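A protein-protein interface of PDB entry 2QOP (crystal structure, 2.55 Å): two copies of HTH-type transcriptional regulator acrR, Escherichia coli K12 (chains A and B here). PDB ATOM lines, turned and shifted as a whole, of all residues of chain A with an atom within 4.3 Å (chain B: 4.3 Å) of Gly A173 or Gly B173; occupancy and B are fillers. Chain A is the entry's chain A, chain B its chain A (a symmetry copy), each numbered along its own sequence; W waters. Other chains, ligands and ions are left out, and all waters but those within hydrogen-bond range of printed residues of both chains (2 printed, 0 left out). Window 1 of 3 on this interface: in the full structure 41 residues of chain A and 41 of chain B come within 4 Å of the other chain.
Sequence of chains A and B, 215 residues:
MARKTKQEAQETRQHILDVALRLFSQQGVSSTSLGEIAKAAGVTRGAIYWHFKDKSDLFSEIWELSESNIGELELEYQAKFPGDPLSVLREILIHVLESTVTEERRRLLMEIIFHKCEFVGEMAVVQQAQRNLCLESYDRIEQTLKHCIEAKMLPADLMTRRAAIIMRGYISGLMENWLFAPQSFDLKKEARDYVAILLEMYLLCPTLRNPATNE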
ATOM      1  N   GLY A 169       4.728 -28.337  -8.557  1.00  0.00           N
ATOM      2  CA  GLY A 169       5.509 -29.151  -9.489  1.00  0.00           C
ATOM      3  C   GLY A 169       5.613 -28.547 -10.879  1.00  0.00           C
ATOM      4  O   GLY A 169       6.650 -28.655 -11.536  1.00  0.00           O
ATOM      5  N   TYR A 170       4.532 -27.907 -11.320  1.00  0.00           N
ATOM      6  CA  TYR A 170       4.469 -27.261 -12.631  1.00  0.00           C
ATOM      7  C   TYR A 170       5.304 -25.980 -12.674  1.00  0.00           C
ATOM      8  O   TYR A 170       5.990 -25.715 -13.663  1.00  0.00           O
ATOM      9  CB  TYR A 170       3.007 -26.968 -12.999  1.00  0.00           C
ATOM     10  CG  TYR A 170       2.798 -26.240 -14.310  1.00  0.00           C
ATOM     11  CD1 TYR A 170       2.699 -26.941 -15.512  1.00  0.00           C
ATOM     12  CD2 TYR A 170       2.677 -24.851 -14.346  1.00  0.00           C
ATOM     13  CE1 TYR A 170       2.497 -26.273 -16.718  1.00  0.00           C
ATOM     14  CE2 TYR A 170       2.475 -24.176 -15.543  1.00  0.00           C
ATOM     15  CZ  TYR A 170       2.386 -24.892 -16.724  1.00  0.00           C
ATOM     16  OH  TYR A 170       2.185 -24.222 -17.908  1.00  0.00           O
ATOM     17  N   ILE A 171       5.238 -25.195 -11.599  1.00  0.00           N
ATOM     18  CA  ILE A 171       5.932 -23.908 -11.522  1.00  0.00           C
ATOM     19  C   ILE A 171       7.436 -24.079 -11.292  1.00  0.00           C
ATOM     20  O   ILE A 171       8.243 -23.558 -12.065  1.00  0.00           O
ATOM     21  CB  ILE A 171       5.298 -22.974 -10.443  1.00  0.00           C
ATOM     22  CG1 ILE A 171       3.830 -22.654 -10.777  1.00  0.00           C
ATOM     23  CG2 ILE A 171       6.121 -21.693 -10.250  1.00  0.00           C
ATOM     24  CD1 ILE A 171       3.586 -21.976 -12.129  1.00  0.00           C
ATOM     25  N   SER A 172       7.803 -24.811 -10.241  1.00  0.00           N
ATOM     26  CA  SER A 172       9.209 -25.047  -9.899  1.00  0.00           C
ATOM     27  C   SER A 172       9.932 -25.913 -10.932  1.00  0.00           C
ATOM     28  O   SER A 172      11.158 -25.856 -11.050  1.00  0.00           O
ATOM     29  CB  SER A 172       9.332 -25.675  -8.507  1.00  0.00           C
ATOM     30  OG  SER A 172       8.794 -24.821  -7.513  1.00  0.00           O
ATOM     31  N   GLY A 173       9.163 -26.711 -11.672  1.00  0.00           N
ATOM     32  CA  GLY A 173       9.699 -27.540 -12.749  1.00  0.00           C
ATOM     33  C   GLY A 173      10.157 -26.724 -13.941  1.00  0.00           C
ATOM     34  O   GLY A 173      11.227 -26.975 -14.497  1.00  0.00           O
ATOM     35  N   LEU A 174       9.343 -25.744 -14.332  1.00  0.00           N
ATOM     36  CA  LEU A 174       9.687 -24.823 -15.417  1.00  0.00           C
ATOM     37  C   LEU A 174      10.803 -23.863 -15.007  1.00  0.00           C
ATOM     38  O   LEU A 174      11.542 -23.360 -15.858  1.00  0.00           O
ATOM     39  CB  LEU A 174       8.453 -24.035 -15.872  1.00  0.00           C
ATOM     40  CG  LEU A 174       7.355 -24.777 -16.644  1.00  0.00           C
ATOM     41  CD1 LEU A 174       6.062 -23.974 -16.637  1.00  0.00           C
ATOM     42  CD2 LEU A 174       7.784 -25.095 -18.073  1.00  0.00           C
ATOM     43  N   MET A 175      10.915 -23.615 -13.704  1.00  0.00           N
ATOM     44  CA  MET A 175      11.969 -22.770 -13.149  1.00  0.00           C
ATOM     45  C   MET A 175      13.324 -23.475 -13.157  1.00  0.00           C
ATOM     46  O   MET A 175      14.329 -22.883 -13.551  1.00  0.00           O
ATOM     47  CB  MET A 175      11.612 -22.324 -11.727  1.00  0.00           C
ATOM     48  CG  MET A 175      10.547 -21.238 -11.658  1.00  0.00           C
ATOM     49  SD  MET A 175       9.793 -21.084 -10.026  1.00  0.00           S
ATOM     50  CE  MET A 175      11.095 -20.268  -9.105  1.00  0.00           C
ATOM     51  N   GLU A 176      13.341 -24.738 -12.732  1.00  0.00           N
ATOM     52  CA  GLU A 176      14.580 -25.519 -12.657  1.00  0.00           C
ATOM     53  C   GLU A 176      15.092 -25.952 -14.034  1.00  0.00           C
ATOM     54  O   GLU A 176      16.289 -26.191 -14.209  1.00  0.00           O
ATOM     55  CB  GLU A 176      14.420 -26.718 -11.707  1.00  0.00           C
ATOM     56  CG  GLU A 176      13.618 -27.907 -12.244  1.00  0.00           C
ATOM     57  CD  GLU A 176      14.491 -28.991 -12.867  1.00  0.00           C
ATOM     58  OE1 GLU A 176      15.734 -28.919 -12.743  1.00  0.00           O
ATOM     59  OE2 GLU A 176      13.929 -29.922 -13.478  1.00  0.00           O
ATOM     60  N   ASN A 177      14.181 -26.051 -15.001  1.00  0.00           N
ATOM     61  CA  ASN A 177      14.536 -26.377 -16.380  1.00  0.00           C
ATOM     62  C   ASN A 177      15.156 -25.194 -17.119  1.00  0.00           C
ATOM     63  O   ASN A 177      16.038 -25.374 -17.961  1.00  0.00           O
ATOM     64  CB  ASN A 177      13.317 -26.896 -17.149  1.00  0.00           C
ATOM     65  CG  ASN A 177      13.087 -28.384 -16.949  1.00  0.00           C
ATOM     66  OD1 ASN A 177      13.184 -29.165 -17.895  1.00  0.00           O
ATOM     67  ND2 ASN A 177      12.789 -28.784 -15.719  1.00  0.00           N
ATOM     68  N   GLY B 169       8.883 -30.039 -17.865  1.00  0.00           N
ATOM     69  CA  GLY B 169       8.741 -29.244 -16.643  1.00  0.00           C
ATOM     70  C   GLY B 169       7.735 -29.821 -15.661  1.00  0.00           C
ATOM     71  O   GLY B 169       7.932 -29.751 -14.447  1.00  0.00           O
ATOM     72  N   TYR B 170       6.658 -30.392 -16.196  1.00  0.00           N
ATOM     73  CA  TYR B 170       5.599 -31.002 -15.393  1.00  0.00           C
ATOM     74  C   TYR B 170       6.050 -32.324 -14.768  1.00  0.00           C
ATOM     75  O   TYR B 170       5.746 -32.601 -13.606  1.00  0.00           O
ATOM     76  CB  TYR B 170       4.344 -31.209 -16.253  1.00  0.00           C
ATOM     77  CG  TYR B 170       3.184 -31.893 -15.560  1.00  0.00           C
ATOM     78  CD1 TYR B 170       2.254 -31.160 -14.824  1.00  0.00           C
ATOM     79  CD2 TYR B 170       3.005 -33.273 -15.661  1.00  0.00           C
ATOM     80  CE1 TYR B 170       1.181 -31.788 -14.195  1.00  0.00           C
ATOM     81  CE2 TYR B 170       1.938 -33.908 -15.037  1.00  0.00           C
ATOM     82  CZ  TYR B 170       1.031 -33.161 -14.306  1.00  0.00           C
ATOM     83  OH  TYR B 170      -0.025 -33.791 -13.691  1.00  0.00           O
ATOM     84  N   ILE B 171       6.771 -33.129 -15.546  1.00  0.00           N
ATOM     85  CA  ILE B 171       7.219 -34.453 -15.107  1.00  0.00           C
ATOM     86  C   ILE B 171       8.392 -34.367 -14.127  1.00  0.00           C
ATOM     87  O   ILE B 171       8.317 -34.910 -13.023  1.00  0.00           O
ATOM     88  CB  ILE B 171       7.562 -35.378 -16.318  1.00  0.00           C
ATOM     89  CG1 ILE B 171       6.327 -35.612 -17.206  1.00  0.00           C
ATOM     90  CG2 ILE B 171       8.181 -36.704 -15.859  1.00  0.00           C
ATOM     91  CD1 ILE B 171       5.116 -36.244 -16.512  1.00  0.00           C
ATOM     92  N   SER B 172       9.461 -33.680 -14.529  1.00  0.00           N
ATOM     93  CA  SER B 172      10.657 -33.527 -13.694  1.00  0.00           C
ATOM     94  C   SER B 172      10.403 -32.676 -12.449  1.00  0.00           C
ATOM     95  O   SER B 172      11.120 -32.794 -11.452  1.00  0.00           O
ATOM     96  CB  SER B 172      11.815 -32.939 -14.507  1.00  0.00           C
ATOM     97  OG  SER B 172      12.161 -33.787 -15.588  1.00  0.00           O
ATOM     98  N   GLY B 173       9.383 -31.821 -12.518  1.00  0.00           N
ATOM     99  CA  GLY B 173       8.973 -30.996 -11.385  1.00  0.00           C
ATOM    100  C   GLY B 173       8.337 -31.806 -10.272  1.00  0.00           C
ATOM    101  O   GLY B 173       8.639 -31.598  -9.096  1.00  0.00           O
ATOM    102  N   LEU B 174       7.456 -32.732 -10.648  1.00  0.00           N
ATOM    103  CA  LEU B 174       6.820 -33.644  -9.695  1.00  0.00           C
ATOM    104  C   LEU B 174       7.813 -34.671  -9.151  1.00  0.00           C
ATOM    105  O   LEU B 174       7.636 -35.192  -8.047  1.00  0.00           O
ATOM    106  CB  LEU B 174       5.624 -34.356 -10.338  1.00  0.00           C
ATOM    107  CG  LEU B 174       4.360 -33.539 -10.634  1.00  0.00           C
ATOM    108  CD1 LEU B 174       3.472 -34.272 -11.628  1.00  0.00           C
ATOM    109  CD2 LEU B 174       3.588 -33.210  -9.361  1.00  0.00           C
ATOM    110  N   MET B 175       8.852 -34.955  -9.935  1.00  0.00           N
ATOM    111  CA  MET B 175       9.918 -35.868  -9.531  1.00  0.00           C
ATOM    112  C   MET B 175      10.842 -35.235  -8.492  1.00  0.00           C
ATOM    113  O   MET B 175      11.179 -35.869  -7.492  1.00  0.00           O
ATOM    114  CB  MET B 175      10.726 -36.328 -10.749  1.00  0.00           C
ATOM    115  CG  MET B 175      10.019 -37.357 -11.618  1.00  0.00           C
ATOM    116  SD  MET B 175      10.738 -37.511 -13.266  1.00  0.00           S
ATOM    117  CE  MET B 175      12.244 -38.416 -12.919  1.00  0.00           C
ATOM    118  N   GLU B 176      11.238 -33.985  -8.730  1.00  0.00           N
ATOM    119  CA  GLU B 176      12.152 -33.272  -7.832  1.00  0.00           C
ATOM    120  C   GLU B 176      11.480 -32.834  -6.527  1.00  0.00           C
ATOM    121  O   GLU B 176      12.150 -32.655  -5.508  1.00  0.00           O
ATOM    122  CB  GLU B 176      12.824 -32.089  -8.551  1.00  0.00           C
ATOM    123  CG  GLU B 176      11.954 -30.847  -8.769  1.00  0.00           C
ATOM    124  CD  GLU B 176      12.119 -29.796  -7.677  1.00  0.00           C
ATOM    125  OE1 GLU B 176      13.028 -29.936  -6.829  1.00  0.00           O
ATOM    126  OE2 GLU B 176      11.339 -28.823  -7.673  1.00  0.00           O
ATOM    127  N   ASN B 177      10.159 -32.664  -6.569  1.00  0.00           N
ATOM    128  CA  ASN B 177       9.376 -32.324  -5.384  1.00  0.00           C
ATOM    129  C   ASN B 177       9.168 -33.521  -4.459  1.00  0.00           C
ATOM    130  O   ASN B 177       9.127 -33.367  -3.236  1.00  0.00           O
ATOM    131  CB  ASN B 177       8.023 -31.724  -5.778  1.00  0.00           C
ATOM    132  CG  ASN B 177       8.100 -30.231  -6.047  1.00  0.00           C
ATOM    133  OD1 ASN B 177       7.495 -29.435  -5.331  1.00  0.00           O
ATOM    134  ND2 ASN B 177       8.846 -29.845  -7.074  1.00  0.00           N
HETATM  135  O   HOH W   1      10.999 -28.164 -19.716  1.00  0.00           O
HETATM  136  O   HOH W   2       4.636 -30.276  -5.790  1.00  0.00           O
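O of Gly B169 lies close to O of Gly A169 (3.4 Å).
The side-chain carboxylate (OE2) of Glu A176 lies within hydrogen-bond range of the side-chain amide nitrogen (ND2) of Asn A177 (2.8 Å). The side-chain amide nitrogen of Asn B177 lies within hydrogen-bond range of the side-chain carboxylate of Glu B176, 2.8 Å away. The backbone carbonyl oxygen (O) of Gly B173 sits at hydrogen-bond distance from the side-chain amide nitrogen (ND2) of Asn B177, 2.7 Å away. ND2 of Asn A177 sits at hydrogen-bond distance from O of Gly A173 (2.7 Å).
Among the printed residues, merely in contact across the chains: Gly A169 with Gly B173, Ser A172 with Glu B176, Gly A173 with Gly B169, Gly A173 with Gly B173 and Glu A176 with Ser B172.
Printed residues of chain B within 4 Å of Gly A173: Gly B169 (3.3 Å) and Gly B173 (3.8 Å). Of the printed residues of chain A, Glu B176 touches Ser A172. Of the printed residues of chain B, Glu A176 touches Ser B172 (3.8 Å). Printed residues of chain A within 4 Å of Gly B169: Gly A169 and Gly A173. Printed residues of chain A within 4 Å of Ser B172: Glu A176 (3.8 Å). Of the printed residues of chain B, Ser A172 touches Glu B176 (3.8 Å). Met B175 touches none of the printed residues of chain A. The nearest printed residue of chain A that does not touch Gly B169 is Asn A177 (4.2 Å).
Among the printed residues, 6 pairs touch across the chains.
Gly A169 touches its own counterpart, Gly B169. Gly A169 touches Gly B173, and with the chains exchanged Gly A173 touches Gly B169. Ser A172 touches Glu B176, and with the chains exchanged Glu A176 touches Ser B172. Gly A173 touches its own counterpart, Gly B173. Of the 6 pairs that touch across the chains among the printed residues, 6 have their exchanged pair printed and touching as well.
Water W2 bridges OD1 of Asn B177 (3.0 Å) and N of Gly A169 (3.4 Å). Water W1 lies within hydrogen-bond range of OD1 of Asn A177 (3.0 Å) and N of Gly B169 (3.4 Å).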
